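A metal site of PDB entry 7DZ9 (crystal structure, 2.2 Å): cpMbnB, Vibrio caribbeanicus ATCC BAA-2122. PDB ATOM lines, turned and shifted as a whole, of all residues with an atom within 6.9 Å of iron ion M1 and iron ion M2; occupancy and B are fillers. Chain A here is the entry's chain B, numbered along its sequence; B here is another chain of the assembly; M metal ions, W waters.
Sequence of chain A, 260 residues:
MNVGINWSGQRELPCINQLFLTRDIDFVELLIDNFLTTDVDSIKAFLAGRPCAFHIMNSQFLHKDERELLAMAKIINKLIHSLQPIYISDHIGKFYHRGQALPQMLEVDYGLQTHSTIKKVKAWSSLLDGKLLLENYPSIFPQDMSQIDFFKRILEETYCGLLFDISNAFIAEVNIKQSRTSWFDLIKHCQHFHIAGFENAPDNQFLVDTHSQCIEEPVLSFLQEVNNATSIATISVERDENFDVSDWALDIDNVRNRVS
OE2 of Glu 135 lies close to ND2 of Asn 168, at 3.4 Å. The backbone NH of Glu 135 lies within hydrogen-bond range of the backbone carbonyl oxygen of Asp 90. OD1 of Asp 165 sits at hydrogen-bond distance from N of Asn 168 (2.8 Å). The side-chain hydroxyl (OG) of Ser 167 sits at hydrogen-bond distance from the side-chain carboxylate (OD1) of Asp 165 (3.1 Å). The backbone NH (N) of Glu 238 lies within hydrogen-bond range of the backbone carbonyl oxygen (O) of Ile 195 (3.0 Å). A ring nitrogen (NE2) of His 194 lies within hydrogen-bond range of the side-chain carboxylate (OE1) of Glu 29 (2.6 Å). The backbone NH of His 194 sits at hydrogen-bond distance from the backbone carbonyl oxygen of Phe 164 (3.0 Å). The backbone NH (N) of Ile 166 is in hydrogen-bond range of the backbone carbonyl oxygen (O) of His 194 (2.8 Å).
Within 4 Å of iron ion M1: His 55, His 91, Glu 135 and Cys 18 of chain B.
Within 4 Å of iron ion M2: Glu 135, Asp 165, His 194 and Glu 238.
Iron ion M1 is bound by water W1, 1.9 Å away. The side-chain carboxylate (OE1) of Glu 135 is bound to iron ion M1 (2.2 Å). Iron ion M1 is bound by NE2 of His 91, at 2.2 Å. NE2 of His 55 binds iron ion M1, at 2.2 Å. Iron ion M1 is bound by water W3 (2.3 Å). Iron ion M1 is bound by SG of Cys 18 of chain B (2.5 Å). Iron ion M1 has six donor atoms within binding distance.
Iron ion M2 is bound by the side-chain carboxylate of Glu 135 (2.0 Å), water W2 (2.0 Å), water W1 (2.1 Å), the side-chain carboxylate of Asp 165 (2.1 Å), the side-chain carboxylate of Glu 238 (2.2 Å) and a ring nitrogen (ND1) of His 194 (2.3 Å).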
ATOM      1  N   GLU A  29     -11.242  27.405 -13.338  1.00  0.00           N
ATOM      2  CA  GLU A  29     -12.318  28.342 -13.602  1.00  0.00           C
ATOM      3  C   GLU A  29     -12.942  28.726 -12.263  1.00  0.00           C
ATOM      4  O   GLU A  29     -13.652  27.928 -11.660  1.00  0.00           O
ATOM      5  CB  GLU A  29     -13.348  27.749 -14.558  1.00  0.00           C
ATOM      6  CG  GLU A  29     -14.397  28.769 -15.021  1.00  0.00           C
ATOM      7  CD  GLU A  29     -15.576  28.097 -15.697  1.00  0.00           C
ATOM      8  OE1 GLU A  29     -15.626  28.110 -16.957  1.00  0.00           O
ATOM      9  OE2 GLU A  29     -16.454  27.552 -14.967  1.00  0.00           O
ATOM     10  N   LEU A  31     -15.603  30.438  -9.929  1.00  0.00           N
ATOM     11  CA  LEU A  31     -16.934  31.039  -9.862  1.00  0.00           C
ATOM     12  C   LEU A  31     -16.734  32.367  -9.147  1.00  0.00           C
ATOM     13  O   LEU A  31     -16.880  32.492  -7.928  1.00  0.00           O
ATOM     14  CB  LEU A  31     -17.919  30.113  -9.157  1.00  0.00           C
ATOM     15  CG  LEU A  31     -19.398  30.244  -9.526  1.00  0.00           C
ATOM     16  CD1 LEU A  31     -19.669  29.989 -11.028  1.00  0.00           C
ATOM     17  CD2 LEU A  31     -20.238  29.303  -8.662  1.00  0.00           C
ATOM     18  N   HIS A  55     -16.073  32.548 -14.192  1.00  0.00           N
ATOM     19  CA  HIS A  55     -17.445  32.141 -14.451  1.00  0.00           C
ATOM     20  C   HIS A  55     -18.316  32.844 -13.427  1.00  0.00           C
ATOM     21  O   HIS A  55     -18.024  32.783 -12.231  1.00  0.00           O
ATOM     22  CB  HIS A  55     -17.548  30.616 -14.348  1.00  0.00           C
ATOM     23  CG  HIS A  55     -18.787  30.018 -14.941  1.00  0.00           C
ATOM     24  ND1 HIS A  55     -19.291  30.387 -16.167  1.00  0.00           N
ATOM     25  CD2 HIS A  55     -19.607  29.043 -14.473  1.00  0.00           C
ATOM     26  CE1 HIS A  55     -20.379  29.691 -16.430  1.00  0.00           C
ATOM     27  NE2 HIS A  55     -20.589  28.860 -15.419  1.00  0.00           N
ATOM     28  N   ILE A  56     -19.372  33.538 -13.871  1.00  0.00           N
ATOM     29  CA  ILE A  56     -20.227  34.331 -12.982  1.00  0.00           C
ATOM     30  C   ILE A  56     -21.575  33.625 -12.834  1.00  0.00           C
ATOM     31  O   ILE A  56     -22.345  33.543 -13.784  1.00  0.00           O
ATOM     32  CB  ILE A  56     -20.427  35.757 -13.516  1.00  0.00           C
ATOM     33  CG1 ILE A  56     -19.078  36.449 -13.707  1.00  0.00           C
ATOM     34  CG2 ILE A  56     -21.353  36.544 -12.607  1.00  0.00           C
ATOM     35  CD1 ILE A  56     -19.162  37.647 -14.637  1.00  0.00           C
ATOM     36  N   MET A  57     -21.892  33.223 -11.605  1.00  0.00           N
ATOM     37  CA  MET A  57     -23.114  32.487 -11.326  1.00  0.00           C
ATOM     38  C   MET A  57     -24.302  33.413 -11.048  1.00  0.00           C
ATOM     39  O   MET A  57     -25.362  33.250 -11.643  1.00  0.00           O
ATOM     40  CB  MET A  57     -22.880  31.544 -10.126  1.00  0.00           C
ATOM     41  CG  MET A  57     -24.128  30.826  -9.593  1.00  0.00           C
ATOM     42  SD  MET A  57     -24.556  29.345 -10.495  1.00  0.00           S
ATOM     43  CE  MET A  57     -25.593  29.970 -11.829  1.00  0.00           C
ATOM     44  N   SER A  89     -17.246  34.810 -18.169  1.00  0.00           N
ATOM     45  CA  SER A  89     -18.459  34.136 -18.626  1.00  0.00           C
ATOM     46  C   SER A  89     -19.590  34.306 -17.601  1.00  0.00           C
ATOM     47  O   SER A  89     -19.343  34.515 -16.424  1.00  0.00           O
ATOM     48  CB  SER A  89     -18.191  32.655 -18.911  1.00  0.00           C
ATOM     49  OG  SER A  89     -17.833  31.956 -17.733  1.00  0.00           O
ATOM     50  N   ASP A  90     -20.821  34.233 -18.088  1.00  0.00           N
ATOM     51  CA  ASP A  90     -21.999  34.338 -17.239  1.00  0.00           C
ATOM     52  C   ASP A  90     -23.054  33.411 -17.809  1.00  0.00           C
ATOM     53  O   ASP A  90     -22.835  32.715 -18.813  1.00  0.00           O
ATOM     54  CB  ASP A  90     -22.462  35.813 -17.164  1.00  0.00           C
ATOM     55  CG  ASP A  90     -23.285  36.136 -15.907  1.00  0.00           C
ATOM     56  OD1 ASP A  90     -24.103  35.303 -15.441  1.00  0.00           O
ATOM     57  OD2 ASP A  90     -23.154  37.272 -15.410  1.00  0.00           O
ATOM     58  N   HIS A  91     -24.229  33.415 -17.186  1.00  0.00           N
ATOM     59  CA  HIS A  91     -25.329  32.534 -17.560  1.00  0.00           C
ATOM     60  C   HIS A  91     -26.491  33.357 -18.065  1.00  0.00           C
ATOM     61  O   HIS A  91     -26.625  34.545 -17.752  1.00  0.00           O
ATOM     62  CB  HIS A  91     -25.833  31.683 -16.400  1.00  0.00           C
ATOM     63  CG  HIS A  91     -24.815  30.779 -15.784  1.00  0.00           C
ATOM     64  ND1 HIS A  91     -23.866  31.217 -14.898  1.00  0.00           N
ATOM     65  CD2 HIS A  91     -24.628  29.444 -15.917  1.00  0.00           C
ATOM     66  CE1 HIS A  91     -23.115  30.203 -14.513  1.00  0.00           C
ATOM     67  NE2 HIS A  91     -23.553  29.114 -15.116  1.00  0.00           N
ATOM     68  N   MET A 105     -31.733  28.503 -10.210  1.00  0.00           N
ATOM     69  CA  MET A 105     -31.699  29.285 -11.444  1.00  0.00           C
ATOM     70  C   MET A 105     -32.498  28.558 -12.521  1.00  0.00           C
ATOM     71  O   MET A 105     -32.182  27.422 -12.901  1.00  0.00           O
ATOM     72  CB  MET A 105     -30.262  29.519 -11.909  1.00  0.00           C
ATOM     73  CG  MET A 105     -30.136  30.319 -13.233  1.00  0.00           C
ATOM     74  SD  MET A 105     -28.435  30.573 -13.877  1.00  0.00           S
ATOM     75  CE  MET A 105     -28.220  29.126 -14.899  1.00  0.00           C
ATOM     76  N   GLU A 135     -23.164  30.956 -21.223  1.00  0.00           N
ATOM     77  CA  GLU A 135     -23.253  29.501 -21.219  1.00  0.00           C
ATOM     78  C   GLU A 135     -24.653  29.036 -21.606  1.00  0.00           C
ATOM     79  O   GLU A 135     -25.643  29.614 -21.170  1.00  0.00           O
ATOM     80  CB  GLU A 135     -22.885  28.967 -19.838  1.00  0.00           C
ATOM     81  CG  GLU A 135     -22.847  27.447 -19.767  1.00  0.00           C
ATOM     82  CD  GLU A 135     -22.479  26.927 -18.386  1.00  0.00           C
ATOM     83  OE1 GLU A 135     -22.537  27.698 -17.401  1.00  0.00           O
ATOM     84  OE2 GLU A 135     -22.125  25.733 -18.277  1.00  0.00           O
ATOM     85  N   ASN A 136     -24.735  27.987 -22.421  1.00  0.00           N
ATOM     86  CA  ASN A 136     -26.021  27.365 -22.732  1.00  0.00           C
ATOM     87  C   ASN A 136     -26.604  26.665 -21.512  1.00  0.00           C
ATOM     88  O   ASN A 136     -25.874  26.059 -20.716  1.00  0.00           O
ATOM     89  CB  ASN A 136     -25.903  26.371 -23.904  1.00  0.00           C
ATOM     90  CG  ASN A 136     -24.797  25.354 -23.716  1.00  0.00           C
ATOM     91  OD1 ASN A 136     -23.623  25.707 -23.573  1.00  0.00           O
ATOM     92  ND2 ASN A 136     -25.163  24.074 -23.735  1.00  0.00           N
ATOM     93  N   LEU A 163     -19.884  30.176 -24.398  1.00  0.00           N
ATOM     94  CA  LEU A 163     -19.182  29.154 -23.618  1.00  0.00           C
ATOM     95  C   LEU A 163     -20.045  27.897 -23.719  1.00  0.00           C
ATOM     96  O   LEU A 163     -21.168  27.877 -23.200  1.00  0.00           O
ATOM     97  CB  LEU A 163     -18.997  29.594 -22.162  1.00  0.00           C
ATOM     98  CG  LEU A 163     -18.501  28.543 -21.153  1.00  0.00           C
ATOM     99  CD1 LEU A 163     -17.052  28.128 -21.425  1.00  0.00           C
ATOM    100  CD2 LEU A 163     -18.605  29.046 -19.705  1.00  0.00           C
ATOM    101  N   PHE A 164     -19.568  26.887 -24.430  1.00  0.00           N
ATOM    102  CA  PHE A 164     -20.452  25.776 -24.782  1.00  0.00           C
ATOM    103  C   PHE A 164     -20.308  24.676 -23.752  1.00  0.00           C
ATOM    104  O   PHE A 164     -19.222  24.133 -23.578  1.00  0.00           O
ATOM    105  CB  PHE A 164     -20.161  25.207 -26.175  1.00  0.00           C
ATOM    106  CG  PHE A 164     -21.133  24.125 -26.585  1.00  0.00           C
ATOM    107  CD1 PHE A 164     -22.474  24.418 -26.776  1.00  0.00           C
ATOM    108  CD2 PHE A 164     -20.694  22.819 -26.777  1.00  0.00           C
ATOM    109  CE1 PHE A 164     -23.395  23.427 -27.151  1.00  0.00           C
ATOM    110  CE2 PHE A 164     -21.596  21.806 -27.158  1.00  0.00           C
ATOM    111  CZ  PHE A 164     -22.956  22.107 -27.342  1.00  0.00           C
ATOM    112  N   ASP A 165     -21.411  24.361 -23.058  1.00  0.00           N
ATOM    113  CA  ASP A 165     -21.425  23.278 -22.089  1.00  0.00           C
ATOM    114  C   ASP A 165     -21.934  22.013 -22.783  1.00  0.00           C
ATOM    115  O   ASP A 165     -23.130  21.898 -23.099  1.00  0.00           O
ATOM    116  CB  ASP A 165     -22.267  23.629 -20.861  1.00  0.00           C
ATOM    117  CG  ASP A 165     -22.032  22.664 -19.725  1.00  0.00           C
ATOM    118  OD1 ASP A 165     -22.242  21.448 -19.939  1.00  0.00           O
ATOM    119  OD2 ASP A 165     -21.660  23.088 -18.611  1.00  0.00           O
ATOM    120  N   ILE A 166     -21.028  21.051 -22.969  1.00  0.00           N
ATOM    121  CA  ILE A 166     -21.334  19.852 -23.758  1.00  0.00           C
ATOM    122  C   ILE A 166     -22.378  18.998 -23.056  1.00  0.00           C
ATOM    123  O   ILE A 166     -23.294  18.463 -23.685  1.00  0.00           O
ATOM    124  CB  ILE A 166     -20.042  19.065 -24.036  1.00  0.00           C
ATOM    125  CG1 ILE A 166     -19.066  19.933 -24.839  1.00  0.00           C
ATOM    126  CG2 ILE A 166     -20.352  17.753 -24.768  1.00  0.00           C
ATOM    127  CD1 ILE A 166     -17.657  19.360 -24.834  1.00  0.00           C
ATOM    128  N   SER A 167     -22.261  18.843 -21.736  1.00  0.00           N
ATOM    129  CA  SER A 167     -23.234  17.995 -21.067  1.00  0.00           C
ATOM    130  C   SER A 167     -24.566  18.711 -20.846  1.00  0.00           C
ATOM    131  O   SER A 167     -25.619  18.060 -20.840  1.00  0.00           O
ATOM    132  CB  SER A 167     -22.665  17.463 -19.745  1.00  0.00           C
ATOM    133  OG  SER A 167     -22.274  18.506 -18.895  1.00  0.00           O
ATOM    134  N   ASN A 168     -24.544  20.042 -20.666  1.00  0.00           N
ATOM    135  CA  ASN A 168     -25.810  20.789 -20.663  1.00  0.00           C
ATOM    136  C   ASN A 168     -26.584  20.568 -21.958  1.00  0.00           C
ATOM    137  O   ASN A 168     -27.808  20.395 -21.941  1.00  0.00           O
ATOM    138  CB  ASN A 168     -25.565  22.280 -20.444  1.00  0.00           C
ATOM    139  CG  ASN A 168     -25.051  22.606 -19.044  1.00  0.00           C
ATOM    140  OD1 ASN A 168     -24.726  21.719 -18.274  1.00  0.00           O
ATOM    141  ND2 ASN A 168     -24.952  23.889 -18.741  1.00  0.00           N
ATOM    142  N   HIS A 194     -17.287  23.423 -21.366  1.00  0.00           N
ATOM    143  CA  HIS A 194     -17.560  22.717 -20.125  1.00  0.00           C
ATOM    144  C   HIS A 194     -17.991  21.292 -20.454  1.00  0.00           C
ATOM    145  O   HIS A 194     -18.592  21.036 -21.497  1.00  0.00           O
ATOM    146  CB  HIS A 194     -18.706  23.352 -19.332  1.00  0.00           C
ATOM    147  CG  HIS A 194     -18.348  24.606 -18.613  1.00  0.00           C
ATOM    148  ND1 HIS A 194     -19.207  25.208 -17.714  1.00  0.00           N
ATOM    149  CD2 HIS A 194     -17.241  25.382 -18.647  1.00  0.00           C
ATOM    150  CE1 HIS A 194     -18.637  26.292 -17.221  1.00  0.00           C
ATOM    151  NE2 HIS A 194     -17.451  26.431 -17.789  1.00  0.00           N
ATOM    152  N   ILE A 195     -17.741  20.380 -19.502  1.00  0.00           N
ATOM    153  CA  ILE A 195     -18.247  19.018 -19.552  1.00  0.00           C
ATOM    154  C   ILE A 195     -18.351  18.501 -18.118  1.00  0.00           C
ATOM    155  O   ILE A 195     -17.503  18.828 -17.276  1.00  0.00           O
ATOM    156  CB  ILE A 195     -17.334  18.118 -20.431  1.00  0.00           C
ATOM    157  CG1 ILE A 195     -18.040  16.832 -20.833  1.00  0.00           C
ATOM    158  CG2 ILE A 195     -15.994  17.852 -19.753  1.00  0.00           C
ATOM    159  CD1 ILE A 195     -17.232  16.032 -21.843  1.00  0.00           C
ATOM    160  N   ALA A 196     -19.403  17.741 -17.828  1.00  0.00           N
ATOM    161  CA  ALA A 196     -19.673  17.334 -16.449  1.00  0.00           C
ATOM    162  C   ALA A 196     -20.628  16.137 -16.426  1.00  0.00           C
ATOM    163  O   ALA A 196     -21.163  15.724 -17.452  1.00  0.00           O
ATOM    164  CB  ALA A 196     -20.259  18.488 -15.644  1.00  0.00           C
ATOM    165  N   ASP A 209     -28.809  18.683 -13.948  1.00  0.00           N
ATOM    166  CA  ASP A 209     -27.424  19.083 -14.225  1.00  0.00           C
ATOM    167  C   ASP A 209     -26.691  19.277 -12.889  1.00  0.00           C
ATOM    168  O   ASP A 209     -26.399  20.387 -12.466  1.00  0.00           O
ATOM    169  CB  ASP A 209     -27.419  20.358 -15.078  1.00  0.00           C
ATOM    170  CG  ASP A 209     -26.011  20.835 -15.420  1.00  0.00           C
ATOM    171  OD1 ASP A 209     -25.150  19.993 -15.728  1.00  0.00           O
ATOM    172  OD2 ASP A 209     -25.787  22.075 -15.403  1.00  0.00           O
ATOM    173  N   HIS A 211     -23.608  18.118 -11.818  1.00  0.00           N
ATOM    174  CA  HIS A 211     -22.139  18.118 -11.742  1.00  0.00           C
ATOM    175  C   HIS A 211     -21.663  17.240 -10.580  1.00  0.00           C
ATOM    176  O   HIS A 211     -20.733  17.592  -9.835  1.00  0.00           O
ATOM    177  CB  HIS A 211     -21.574  19.538 -11.579  1.00  0.00           C
ATOM    178  CG  HIS A 211     -22.020  20.509 -12.635  1.00  0.00           C
ATOM    179  ND1 HIS A 211     -21.897  21.873 -12.488  1.00  0.00           N
ATOM    180  CD2 HIS A 211     -22.566  20.312 -13.869  1.00  0.00           C
ATOM    181  CE1 HIS A 211     -22.370  22.477 -13.569  1.00  0.00           C
ATOM    182  NE2 HIS A 211     -22.779  21.554 -14.414  1.00  0.00           N
ATOM    183  N   SER A 236     -13.388  22.908 -19.090  1.00  0.00           N
ATOM    184  CA  SER A 236     -13.444  22.780 -17.654  1.00  0.00           C
ATOM    185  C   SER A 236     -14.287  21.542 -17.317  1.00  0.00           C
ATOM    186  O   SER A 236     -15.429  21.425 -17.773  1.00  0.00           O
ATOM    187  CB  SER A 236     -14.044  24.045 -17.020  1.00  0.00           C
ATOM    188  OG  SER A 236     -14.380  23.851 -15.660  1.00  0.00           O
ATOM    189  N   GLU A 238     -16.310  19.934 -14.738  1.00  0.00           N
ATOM    190  CA  GLU A 238     -16.956  20.507 -13.565  1.00  0.00           C
ATOM    191  C   GLU A 238     -17.332  19.446 -12.534  1.00  0.00           C
ATOM    192  O   GLU A 238     -17.746  18.333 -12.882  1.00  0.00           O
ATOM    193  CB  GLU A 238     -18.212  21.284 -13.952  1.00  0.00           C
ATOM    194  CG  GLU A 238     -18.157  22.029 -15.276  1.00  0.00           C
ATOM    195  CD  GLU A 238     -19.325  22.999 -15.402  1.00  0.00           C
ATOM    196  OE1 GLU A 238     -20.295  22.705 -16.106  1.00  0.00           O
ATOM    197  OE2 GLU A 238     -19.290  24.040 -14.736  1.00  0.00           O
ATOM    198  N   THR B  17     -23.486  27.122  -6.373  1.00  0.00           N
ATOM    199  CA  THR B  17     -22.778  26.330  -7.350  1.00  0.00           C
ATOM    200  C   THR B  17     -23.599  26.309  -8.635  1.00  0.00           C
ATOM    201  O   THR B  17     -24.783  26.665  -8.631  1.00  0.00           O
ATOM    202  CB  THR B  17     -22.528  24.882  -6.864  1.00  0.00           C
ATOM    203  OG1 THR B  17     -23.770  24.268  -6.495  1.00  0.00           O
ATOM    204  CG2 THR B  17     -21.587  24.865  -5.640  1.00  0.00           C
ATOM    205  N   CYS B  18     -22.951  25.920  -9.739  1.00  0.00           N
ATOM    206  CA  CYS B  18     -23.706  25.763 -10.971  1.00  0.00           C
ATOM    207  C   CYS B  18     -24.523  24.479 -10.930  1.00  0.00           C
ATOM    208  O   CYS B  18     -25.560  24.385 -11.582  1.00  0.00           O
ATOM    209  CB  CYS B  18     -22.779  25.686 -12.179  1.00  0.00           C
ATOM    210  SG  CYS B  18     -22.145  27.229 -12.745  1.00  0.00           S
ATOM    211  N   GLY B  19     -24.070  23.511 -10.149  1.00  0.00           N
ATOM    212  CA  GLY B  19     -24.769  22.262  -9.971  1.00  0.00           C
ATOM    213  C   GLY B  19     -26.179  22.424  -9.440  1.00  0.00           C
ATOM    214  O   GLY B  19     -26.392  23.016  -8.371  1.00  0.00           O
HETATM  215 FE    FE M   1     -22.263  27.375 -15.275  1.00  0.00          FE
HETATM  216 FE    FE M   2     -21.290  24.410 -17.058  1.00  0.00          FE
HETATM  217 FE    FE M   3     -23.789  21.868 -16.302  1.00  0.00          FE
HETATM  218  O   HOH W   1     -21.310  25.740 -15.471  1.00  0.00           O
HETATM  219  O   HOH W   2     -23.181  23.988 -16.544  1.00  0.00           O
HETATM  220  O   HOH W   3     -24.246  26.226 -15.276  1.00  0.00           O
